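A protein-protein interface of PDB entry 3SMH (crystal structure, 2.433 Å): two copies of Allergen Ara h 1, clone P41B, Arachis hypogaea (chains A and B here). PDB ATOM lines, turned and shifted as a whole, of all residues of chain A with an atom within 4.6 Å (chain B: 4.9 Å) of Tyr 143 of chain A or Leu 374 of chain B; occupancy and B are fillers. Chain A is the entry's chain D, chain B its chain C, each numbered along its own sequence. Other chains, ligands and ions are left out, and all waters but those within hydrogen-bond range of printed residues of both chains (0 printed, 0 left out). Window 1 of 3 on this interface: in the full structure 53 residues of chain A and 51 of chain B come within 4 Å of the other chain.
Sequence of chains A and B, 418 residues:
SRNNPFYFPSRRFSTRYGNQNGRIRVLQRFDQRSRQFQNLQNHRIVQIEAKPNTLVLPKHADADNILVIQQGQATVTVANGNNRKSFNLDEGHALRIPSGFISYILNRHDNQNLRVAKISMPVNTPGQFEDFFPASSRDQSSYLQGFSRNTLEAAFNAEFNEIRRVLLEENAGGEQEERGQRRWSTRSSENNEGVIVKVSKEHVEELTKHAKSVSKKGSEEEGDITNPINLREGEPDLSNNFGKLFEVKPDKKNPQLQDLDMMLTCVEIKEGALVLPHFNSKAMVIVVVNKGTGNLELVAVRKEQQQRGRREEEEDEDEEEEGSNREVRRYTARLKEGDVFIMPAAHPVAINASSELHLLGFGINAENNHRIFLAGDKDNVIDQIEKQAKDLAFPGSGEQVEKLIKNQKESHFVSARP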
ATOM      1  N   HIS A  60     -17.823 -26.527 -24.350  1.00  0.00           N
ATOM      2  CA  HIS A  60     -17.009 -25.804 -25.318  1.00  0.00           C
ATOM      3  C   HIS A  60     -15.999 -24.958 -24.572  1.00  0.00           C
ATOM      4  O   HIS A  60     -16.182 -24.675 -23.400  1.00  0.00           O
ATOM      5  CB  HIS A  60     -17.850 -24.957 -26.281  1.00  0.00           C
ATOM      6  CG  HIS A  60     -18.380 -23.682 -25.688  1.00  0.00           C
ATOM      7  ND1 HIS A  60     -19.669 -23.563 -25.204  1.00  0.00           N
ATOM      8  CD2 HIS A  60     -17.813 -22.458 -25.544  1.00  0.00           C
ATOM      9  CE1 HIS A  60     -19.863 -22.326 -24.773  1.00  0.00           C
ATOM     10  NE2 HIS A  60     -18.751 -21.639 -24.964  1.00  0.00           N
ATOM     11  N   PHE A 132     -16.878 -24.374 -20.886  1.00  0.00           N
ATOM     12  CA  PHE A 132     -18.243 -23.922 -20.676  1.00  0.00           C
ATOM     13  C   PHE A 132     -19.184 -25.107 -20.812  1.00  0.00           C
ATOM     14  O   PHE A 132     -19.455 -25.547 -21.926  1.00  0.00           O
ATOM     15  CB  PHE A 132     -18.618 -22.850 -21.707  1.00  0.00           C
ATOM     16  CG  PHE A 132     -17.955 -21.529 -21.477  1.00  0.00           C
ATOM     17  CD1 PHE A 132     -16.609 -21.359 -21.774  1.00  0.00           C
ATOM     18  CD2 PHE A 132     -18.667 -20.451 -20.969  1.00  0.00           C
ATOM     19  CE1 PHE A 132     -15.986 -20.147 -21.550  1.00  0.00           C
ATOM     20  CE2 PHE A 132     -18.044 -19.228 -20.750  1.00  0.00           C
ATOM     21  CZ  PHE A 132     -16.707 -19.082 -21.039  1.00  0.00           C
ATOM     22  N   PHE A 133     -19.683 -25.606 -19.683  1.00  0.00           N
ATOM     23  CA  PHE A 133     -20.608 -26.750 -19.654  1.00  0.00           C
ATOM     24  C   PHE A 133     -22.066 -26.316 -19.648  1.00  0.00           C
ATOM     25  O   PHE A 133     -22.458 -25.512 -18.809  1.00  0.00           O
ATOM     26  CB  PHE A 133     -20.359 -27.588 -18.401  1.00  0.00           C
ATOM     27  CG  PHE A 133     -18.998 -28.217 -18.347  1.00  0.00           C
ATOM     28  CD1 PHE A 133     -17.915 -27.520 -17.832  1.00  0.00           C
ATOM     29  CD2 PHE A 133     -18.798 -29.514 -18.798  1.00  0.00           C
ATOM     30  CE1 PHE A 133     -16.652 -28.106 -17.771  1.00  0.00           C
ATOM     31  CE2 PHE A 133     -17.538 -30.094 -18.749  1.00  0.00           C
ATOM     32  CZ  PHE A 133     -16.469 -29.382 -18.232  1.00  0.00           C
ATOM     33  N   PRO A 134     -22.881 -26.854 -20.567  1.00  0.00           N
ATOM     34  CA  PRO A 134     -24.316 -26.529 -20.581  1.00  0.00           C
ATOM     35  C   PRO A 134     -25.062 -27.140 -19.398  1.00  0.00           C
ATOM     36  O   PRO A 134     -26.130 -26.657 -19.019  1.00  0.00           O
ATOM     37  CB  PRO A 134     -24.811 -27.132 -21.902  1.00  0.00           C
ATOM     38  CG  PRO A 134     -23.828 -28.183 -22.222  1.00  0.00           C
ATOM     39  CD  PRO A 134     -22.497 -27.688 -21.712  1.00  0.00           C
ATOM     40  N   SER A 141     -21.143 -25.332 -12.366  1.00  0.00           N
ATOM     41  CA  SER A 141     -22.534 -25.041 -12.696  1.00  0.00           C
ATOM     42  C   SER A 141     -22.734 -24.826 -14.194  1.00  0.00           C
ATOM     43  O   SER A 141     -21.820 -24.412 -14.890  1.00  0.00           O
ATOM     44  CB  SER A 141     -23.015 -23.809 -11.926  1.00  0.00           C
ATOM     45  OG  SER A 141     -22.987 -24.044 -10.530  1.00  0.00           O
ATOM     46  N   SER A 142     -23.930 -25.125 -14.683  1.00  0.00           N
ATOM     47  CA  SER A 142     -24.298 -24.792 -16.048  1.00  0.00           C
ATOM     48  C   SER A 142     -24.199 -23.284 -16.241  1.00  0.00           C
ATOM     49  O   SER A 142     -24.576 -22.517 -15.356  1.00  0.00           O
ATOM     50  CB  SER A 142     -25.729 -25.263 -16.329  1.00  0.00           C
ATOM     51  OG  SER A 142     -26.306 -24.571 -17.424  1.00  0.00           O
ATOM     52  N   TYR A 143     -23.691 -22.854 -17.392  1.00  0.00           N
ATOM     53  CA  TYR A 143     -23.606 -21.422 -17.657  1.00  0.00           C
ATOM     54  C   TYR A 143     -25.009 -20.847 -17.842  1.00  0.00           C
ATOM     55  O   TYR A 143     -25.198 -19.640 -17.799  1.00  0.00           O
ATOM     56  CB  TYR A 143     -22.689 -21.091 -18.847  1.00  0.00           C
ATOM     57  CG  TYR A 143     -22.933 -21.908 -20.091  1.00  0.00           C
ATOM     58  CD1 TYR A 143     -24.058 -21.702 -20.870  1.00  0.00           C
ATOM     59  CD2 TYR A 143     -22.026 -22.888 -20.495  1.00  0.00           C
ATOM     60  CE1 TYR A 143     -24.292 -22.454 -22.017  1.00  0.00           C
ATOM     61  CE2 TYR A 143     -22.260 -23.640 -21.640  1.00  0.00           C
ATOM     62  CZ  TYR A 143     -23.393 -23.417 -22.391  1.00  0.00           C
ATOM     63  OH  TYR A 143     -23.637 -24.149 -23.520  1.00  0.00           O
ATOM     64  N   LEU A 144     -25.996 -21.717 -18.040  1.00  0.00           N
ATOM     65  CA  LEU A 144     -27.358 -21.240 -18.210  1.00  0.00           C
ATOM     66  C   LEU A 144     -27.845 -20.622 -16.899  1.00  0.00           C
ATOM     67  O   LEU A 144     -28.708 -19.750 -16.898  1.00  0.00           O
ATOM     68  CB  LEU A 144     -28.281 -22.353 -18.676  1.00  0.00           C
ATOM     69  CG  LEU A 144     -28.067 -22.881 -20.087  1.00  0.00           C
ATOM     70  CD1 LEU A 144     -28.939 -24.086 -20.306  1.00  0.00           C
ATOM     71  CD2 LEU A 144     -28.361 -21.818 -21.115  1.00  0.00           C
ATOM     72  N   GLN A 145     -27.256 -21.054 -15.786  1.00  0.00           N
ATOM     73  CA  GLN A 145     -27.583 -20.483 -14.480  1.00  0.00           C
ATOM     74  C   GLN A 145     -27.148 -19.024 -14.344  1.00  0.00           C
ATOM     75  O   GLN A 145     -27.502 -18.348 -13.382  1.00  0.00           O
ATOM     76  CB  GLN A 145     -26.937 -21.293 -13.354  1.00  0.00           C
ATOM     77  CG  GLN A 145     -27.596 -22.612 -13.068  1.00  0.00           C
ATOM     78  CD  GLN A 145     -26.972 -23.294 -11.868  1.00  0.00           C
ATOM     79  OE1 GLN A 145     -26.119 -22.717 -11.193  1.00  0.00           O
ATOM     80  NE2 GLN A 145     -27.394 -24.527 -11.594  1.00  0.00           N
ATOM     81  N   GLY A 146     -26.354 -18.550 -15.285  1.00  0.00           N
ATOM     82  CA  GLY A 146     -25.872 -17.187 -15.236  1.00  0.00           C
ATOM     83  C   GLY A 146     -26.917 -16.206 -15.733  1.00  0.00           C
ATOM     84  O   GLY A 146     -26.804 -14.992 -15.519  1.00  0.00           O
ATOM     85  N   PHE A 147     -27.930 -16.730 -16.413  1.00  0.00           N
ATOM     86  CA  PHE A 147     -28.996 -15.883 -16.939  1.00  0.00           C
ATOM     87  C   PHE A 147     -30.110 -15.736 -15.905  1.00  0.00           C
ATOM     88  O   PHE A 147     -30.221 -16.549 -15.006  1.00  0.00           O
ATOM     89  CB  PHE A 147     -29.526 -16.422 -18.277  1.00  0.00           C
ATOM     90  CG  PHE A 147     -28.532 -16.312 -19.406  1.00  0.00           C
ATOM     91  CD1 PHE A 147     -27.882 -17.431 -19.877  1.00  0.00           C
ATOM     92  CD2 PHE A 147     -28.236 -15.086 -19.969  1.00  0.00           C
ATOM     93  CE1 PHE A 147     -26.965 -17.341 -20.909  1.00  0.00           C
ATOM     94  CE2 PHE A 147     -27.311 -14.984 -21.002  1.00  0.00           C
ATOM     95  CZ  PHE A 147     -26.677 -16.123 -21.468  1.00  0.00           C
ATOM     96  N   PHE A 156     -36.629 -20.128 -23.205  1.00  0.00           N
ATOM     97  CA  PHE A 156     -37.078 -21.501 -23.383  1.00  0.00           C
ATOM     98  C   PHE A 156     -38.588 -21.648 -23.533  1.00  0.00           C
ATOM     99  O   PHE A 156     -39.072 -22.738 -23.856  1.00  0.00           O
ATOM    100  CB  PHE A 156     -36.549 -22.394 -22.259  1.00  0.00           C
ATOM    101  CG  PHE A 156     -35.068 -22.625 -22.328  1.00  0.00           C
ATOM    102  CD1 PHE A 156     -34.549 -23.624 -23.129  1.00  0.00           C
ATOM    103  CD2 PHE A 156     -34.195 -21.828 -21.615  1.00  0.00           C
ATOM    104  CE1 PHE A 156     -33.182 -23.820 -23.211  1.00  0.00           C
ATOM    105  CE2 PHE A 156     -32.831 -22.021 -21.687  1.00  0.00           C
ATOM    106  CZ  PHE A 156     -32.322 -23.015 -22.487  1.00  0.00           C
ATOM    107  N   PRO B 277     -29.925 -16.153 -25.352  1.00  0.00           N
ATOM    108  CA  PRO B 277     -28.555 -16.526 -24.970  1.00  0.00           C
ATOM    109  C   PRO B 277     -27.810 -17.129 -26.156  1.00  0.00           C
ATOM    110  O   PRO B 277     -28.316 -18.066 -26.801  1.00  0.00           O
ATOM    111  CB  PRO B 277     -28.769 -17.594 -23.880  1.00  0.00           C
ATOM    112  CG  PRO B 277     -30.065 -17.174 -23.222  1.00  0.00           C
ATOM    113  CD  PRO B 277     -30.922 -16.578 -24.353  1.00  0.00           C
ATOM    114  N   HIS B 278     -26.623 -16.595 -26.436  1.00  0.00           N
ATOM    115  CA  HIS B 278     -25.869 -16.989 -27.611  1.00  0.00           C
ATOM    116  C   HIS B 278     -24.445 -16.493 -27.453  1.00  0.00           C
ATOM    117  O   HIS B 278     -24.141 -15.759 -26.510  1.00  0.00           O
ATOM    118  CB  HIS B 278     -26.486 -16.368 -28.862  1.00  0.00           C
ATOM    119  CG  HIS B 278     -26.225 -14.901 -28.980  1.00  0.00           C
ATOM    120  ND1 HIS B 278     -26.791 -13.979 -28.125  1.00  0.00           N
ATOM    121  CD2 HIS B 278     -25.447 -14.196 -29.835  1.00  0.00           C
ATOM    122  CE1 HIS B 278     -26.381 -12.765 -28.458  1.00  0.00           C
ATOM    123  NE2 HIS B 278     -25.566 -12.869 -29.492  1.00  0.00           N
ATOM    124  N   PHE B 279     -23.577 -16.892 -28.379  1.00  0.00           N
ATOM    125  CA  PHE B 279     -22.204 -16.405 -28.387  1.00  0.00           C
ATOM    126  C   PHE B 279     -21.586 -16.519 -29.772  1.00  0.00           C
ATOM    127  O   PHE B 279     -22.079 -17.256 -30.623  1.00  0.00           O
ATOM    128  CB  PHE B 279     -21.344 -17.131 -27.346  1.00  0.00           C
ATOM    129  CG  PHE B 279     -21.319 -18.632 -27.504  1.00  0.00           C
ATOM    130  CD1 PHE B 279     -22.104 -19.439 -26.703  1.00  0.00           C
ATOM    131  CD2 PHE B 279     -20.495 -19.232 -28.451  1.00  0.00           C
ATOM    132  CE1 PHE B 279     -22.080 -20.809 -26.845  1.00  0.00           C
ATOM    133  CE2 PHE B 279     -20.469 -20.603 -28.589  1.00  0.00           C
ATOM    134  CZ  PHE B 279     -21.261 -21.389 -27.783  1.00  0.00           C
ATOM    135  N   VAL B 299     -22.234 -13.965 -19.451  1.00  0.00           N
ATOM    136  CA  VAL B 299     -21.927 -15.068 -18.553  1.00  0.00           C
ATOM    137  C   VAL B 299     -20.508 -15.532 -18.795  1.00  0.00           C
ATOM    138  O   VAL B 299     -20.084 -15.663 -19.940  1.00  0.00           O
ATOM    139  CB  VAL B 299     -22.923 -16.247 -18.732  1.00  0.00           C
ATOM    140  CG1 VAL B 299     -22.445 -17.468 -17.971  1.00  0.00           C
ATOM    141  CG2 VAL B 299     -24.312 -15.851 -18.276  1.00  0.00           C
ATOM    142  N   VAL B 328     -19.580 -19.929 -12.153  1.00  0.00           N
ATOM    143  CA  VAL B 328     -20.201 -19.145 -13.204  1.00  0.00           C
ATOM    144  C   VAL B 328     -20.439 -17.728 -12.685  1.00  0.00           C
ATOM    145  O   VAL B 328     -21.024 -17.541 -11.623  1.00  0.00           O
ATOM    146  CB  VAL B 328     -21.523 -19.800 -13.677  1.00  0.00           C
ATOM    147  CG1 VAL B 328     -22.262 -18.902 -14.633  1.00  0.00           C
ATOM    148  CG2 VAL B 328     -21.235 -21.142 -14.336  1.00  0.00           C
ATOM    149  N   PRO B 348     -21.515 -16.752 -23.252  1.00  0.00           N
ATOM    150  CA  PRO B 348     -22.957 -16.578 -23.510  1.00  0.00           C
ATOM    151  C   PRO B 348     -23.480 -15.178 -23.133  1.00  0.00           C
ATOM    152  O   PRO B 348     -23.153 -14.617 -22.081  1.00  0.00           O
ATOM    153  CB  PRO B 348     -23.613 -17.659 -22.643  1.00  0.00           C
ATOM    154  CG  PRO B 348     -22.567 -18.667 -22.424  1.00  0.00           C
ATOM    155  CD  PRO B 348     -21.253 -17.890 -22.363  1.00  0.00           C
ATOM    156  N   ILE B 372     -23.665 -18.742 -32.254  1.00  0.00           N
ATOM    157  CA  ILE B 372     -24.283 -19.958 -31.778  1.00  0.00           C
ATOM    158  C   ILE B 372     -25.288 -19.662 -30.663  1.00  0.00           C
ATOM    159  O   ILE B 372     -25.001 -18.916 -29.720  1.00  0.00           O
ATOM    160  CB  ILE B 372     -23.213 -20.976 -31.336  1.00  0.00           C
ATOM    161  CG1 ILE B 372     -22.431 -21.487 -32.573  1.00  0.00           C
ATOM    162  CG2 ILE B 372     -23.846 -22.105 -30.536  1.00  0.00           C
ATOM    163  CD1 ILE B 372     -21.281 -22.438 -32.247  1.00  0.00           C
ATOM    164  N   PHE B 373     -26.477 -20.243 -30.788  1.00  0.00           N
ATOM    165  CA  PHE B 373     -27.527 -20.040 -29.801  1.00  0.00           C
ATOM    166  C   PHE B 373     -27.704 -21.200 -28.815  1.00  0.00           C
ATOM    167  O   PHE B 373     -27.275 -22.334 -29.068  1.00  0.00           O
ATOM    168  CB  PHE B 373     -28.835 -19.646 -30.485  1.00  0.00           C
ATOM    169  CG  PHE B 373     -28.806 -18.239 -31.053  1.00  0.00           C
ATOM    170  CD1 PHE B 373     -29.477 -17.202 -30.421  1.00  0.00           C
ATOM    171  CD2 PHE B 373     -28.060 -17.948 -32.195  1.00  0.00           C
ATOM    172  CE1 PHE B 373     -29.441 -15.908 -30.934  1.00  0.00           C
ATOM    173  CE2 PHE B 373     -28.020 -16.649 -32.713  1.00  0.00           C
ATOM    174  CZ  PHE B 373     -28.719 -15.628 -32.075  1.00  0.00           C
ATOM    175  N   LEU B 374     -28.311 -20.887 -27.673  1.00  0.00           N
ATOM    176  CA  LEU B 374     -28.421 -21.825 -26.567  1.00  0.00           C
ATOM    177  C   LEU B 374     -29.893 -22.105 -26.257  1.00  0.00           C
ATOM    178  O   LEU B 374     -30.207 -22.847 -25.331  1.00  0.00           O
ATOM    179  CB  LEU B 374     -27.727 -21.277 -25.319  1.00  0.00           C
ATOM    180  CG  LEU B 374     -26.223 -21.034 -25.441  1.00  0.00           C
ATOM    181  CD1 LEU B 374     -25.680 -20.248 -24.234  1.00  0.00           C
ATOM    182  CD2 LEU B 374     -25.495 -22.347 -25.638  1.00  0.00           C
ATOM    183  N   ALA B 375     -30.782 -21.508 -27.040  1.00  0.00           N
ATOM    184  CA  ALA B 375     -32.218 -21.750 -26.944  1.00  0.00           C
ATOM    185  C   ALA B 375     -32.837 -21.450 -28.297  1.00  0.00           C
ATOM    186  O   ALA B 375     -32.200 -20.877 -29.176  1.00  0.00           O
ATOM    187  CB  ALA B 375     -32.836 -20.867 -25.888  1.00  0.00           C
ATOM    188  N   GLY B 376     -34.086 -21.827 -28.471  1.00  0.00           N
ATOM    189  CA  GLY B 376     -34.745 -21.617 -29.741  1.00  0.00           C
ATOM    190  C   GLY B 376     -34.539 -22.770 -30.697  1.00  0.00           C
ATOM    191  O   GLY B 376     -33.866 -23.747 -30.386  1.00  0.00           O
ATOM    192  N   ASN B 380     -29.300 -23.588 -32.467  1.00  0.00           N
ATOM    193  CA  ASN B 380     -29.246 -24.051 -31.081  1.00  0.00           C
ATOM    194  C   ASN B 380     -28.277 -25.214 -30.937  1.00  0.00           C
ATOM    195  O   ASN B 380     -28.602 -26.330 -31.336  1.00  0.00           O
ATOM    196  CB  ASN B 380     -30.645 -24.512 -30.645  1.00  0.00           C
ATOM    197  CG  ASN B 380     -30.722 -24.844 -29.158  1.00  0.00           C
ATOM    198  OD1 ASN B 380     -29.726 -25.219 -28.535  1.00  0.00           O
ATOM    199  ND2 ASN B 380     -31.911 -24.694 -28.583  1.00  0.00           N
ATOM    200  N   VAL B 381     -27.099 -24.966 -30.371  1.00  0.00           N
ATOM    201  CA  VAL B 381     -26.087 -26.016 -30.254  1.00  0.00           C
ATOM    202  C   VAL B 381     -26.456 -27.100 -29.224  1.00  0.00           C
ATOM    203  O   VAL B 381     -26.108 -28.274 -29.399  1.00  0.00           O
ATOM    204  CB  VAL B 381     -24.703 -25.443 -29.922  1.00  0.00           C
ATOM    205  CG1 VAL B 381     -24.701 -24.787 -28.542  1.00  0.00           C
ATOM    206  CG2 VAL B 381     -23.639 -26.527 -30.017  1.00  0.00           C
ATOM    207  N   ILE B 382     -27.143 -26.703 -28.154  1.00  0.00           N
ATOM    208  CA  ILE B 382     -27.569 -27.661 -27.131  1.00  0.00           C
ATOM    209  C   ILE B 382     -28.450 -28.737 -27.765  1.00  0.00           C
ATOM    210  O   ILE B 382     -28.364 -29.922 -27.426  1.00  0.00           O
ATOM    211  CB  ILE B 382     -28.295 -26.966 -25.946  1.00  0.00           C
ATOM    212  CG1 ILE B 382     -27.295 -26.130 -25.160  1.00  0.00           C
ATOM    213  CG2 ILE B 382     -28.917 -27.985 -25.013  1.00  0.00           C
ATOM    214  CD1 ILE B 382     -27.897 -25.332 -24.080  1.00  0.00           C
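The backbone carbonyl oxygen (O) of Phe 279 of chain B is in hydrogen-bond range of the backbone NH (N) of Ile 372 of chain B (2.7 Å). The backbone carbonyl oxygen (O) of Pro 348 of chain B is in hydrogen-bond range of the backbone NH (N) of Val 299 of chain B (2.9 Å). N of Phe 132 of chain A is in hydrogen-bond range of O of His 60 of chain A, at 2.6 Å. OG of Ser 142 of chain A sits at hydrogen-bond distance from O of Pro 134 of chain A. OE1 of Gln 145 of chain A lies close to OG of Ser 141 of chain A (3.5 Å). The side-chain hydroxyl (OG) of Ser 142 of chain A lies within hydrogen-bond range of the backbone NH (N) of Leu 144 of chain A.
Of the 12 printed residues of chain A, 8 touch a printed residue of chain B. Among the printed residues, no Asp or Glu carboxylate lies within 4 Å of a Lys or Arg side-chain nitrogen of the other chain.
Tyr 143 of chain A touches just these residues of chain B: Val 299 (3.5 Å), Pro 348 (3.7 Å) and Leu 374 (3.3 Å). Of chain A, only Tyr 143 and Phe 156 come within 4 Å of Leu 374 of chain B. Of the printed residues of chain A, Pro 277 of chain B touches Phe 147. Of the printed residues of chain B, Ser 142 of chain A touches Val 328 (3.8 Å). Leu 144 of chain A touches none of the printed residues of chain B. The nearest residue of chain A that does not touch Leu 374 of chain B is Leu 144 of chain A (4.3 Å).
No position is printed for both chains.
Among the printed residues, pairs that only touch across the chains: Tyr 143 of chain A with Leu 374 of chain B (3.3 Å), Ser 141 of chain A with Val 328 of chain B (3.4 Å), His 60 of chain A with Phe 279 of chain B (3.4 Å), Phe 147 of chain A with Pro 277 of chain B (3.5 Å), Tyr 143 of chain A with Val 299 of chain B (3.5 Å), Phe 156 of chain A with Leu 374 of chain B (3.5 Å), Phe 147 of chain A with Pro 348 of chain B (3.6 Å), Gly 146 of chain A with Val 299 of chain B (3.7 Å), Tyr 143 of chain A with Pro 348 of chain B (3.7 Å), Ser 142 of chain A with Val 328 of chain B (3.8 Å), Phe 132 of chain A with Pro 348 of chain B (3.8 Å) and Phe 147 of chain A with Val 299 of chain B (3.98 Å).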
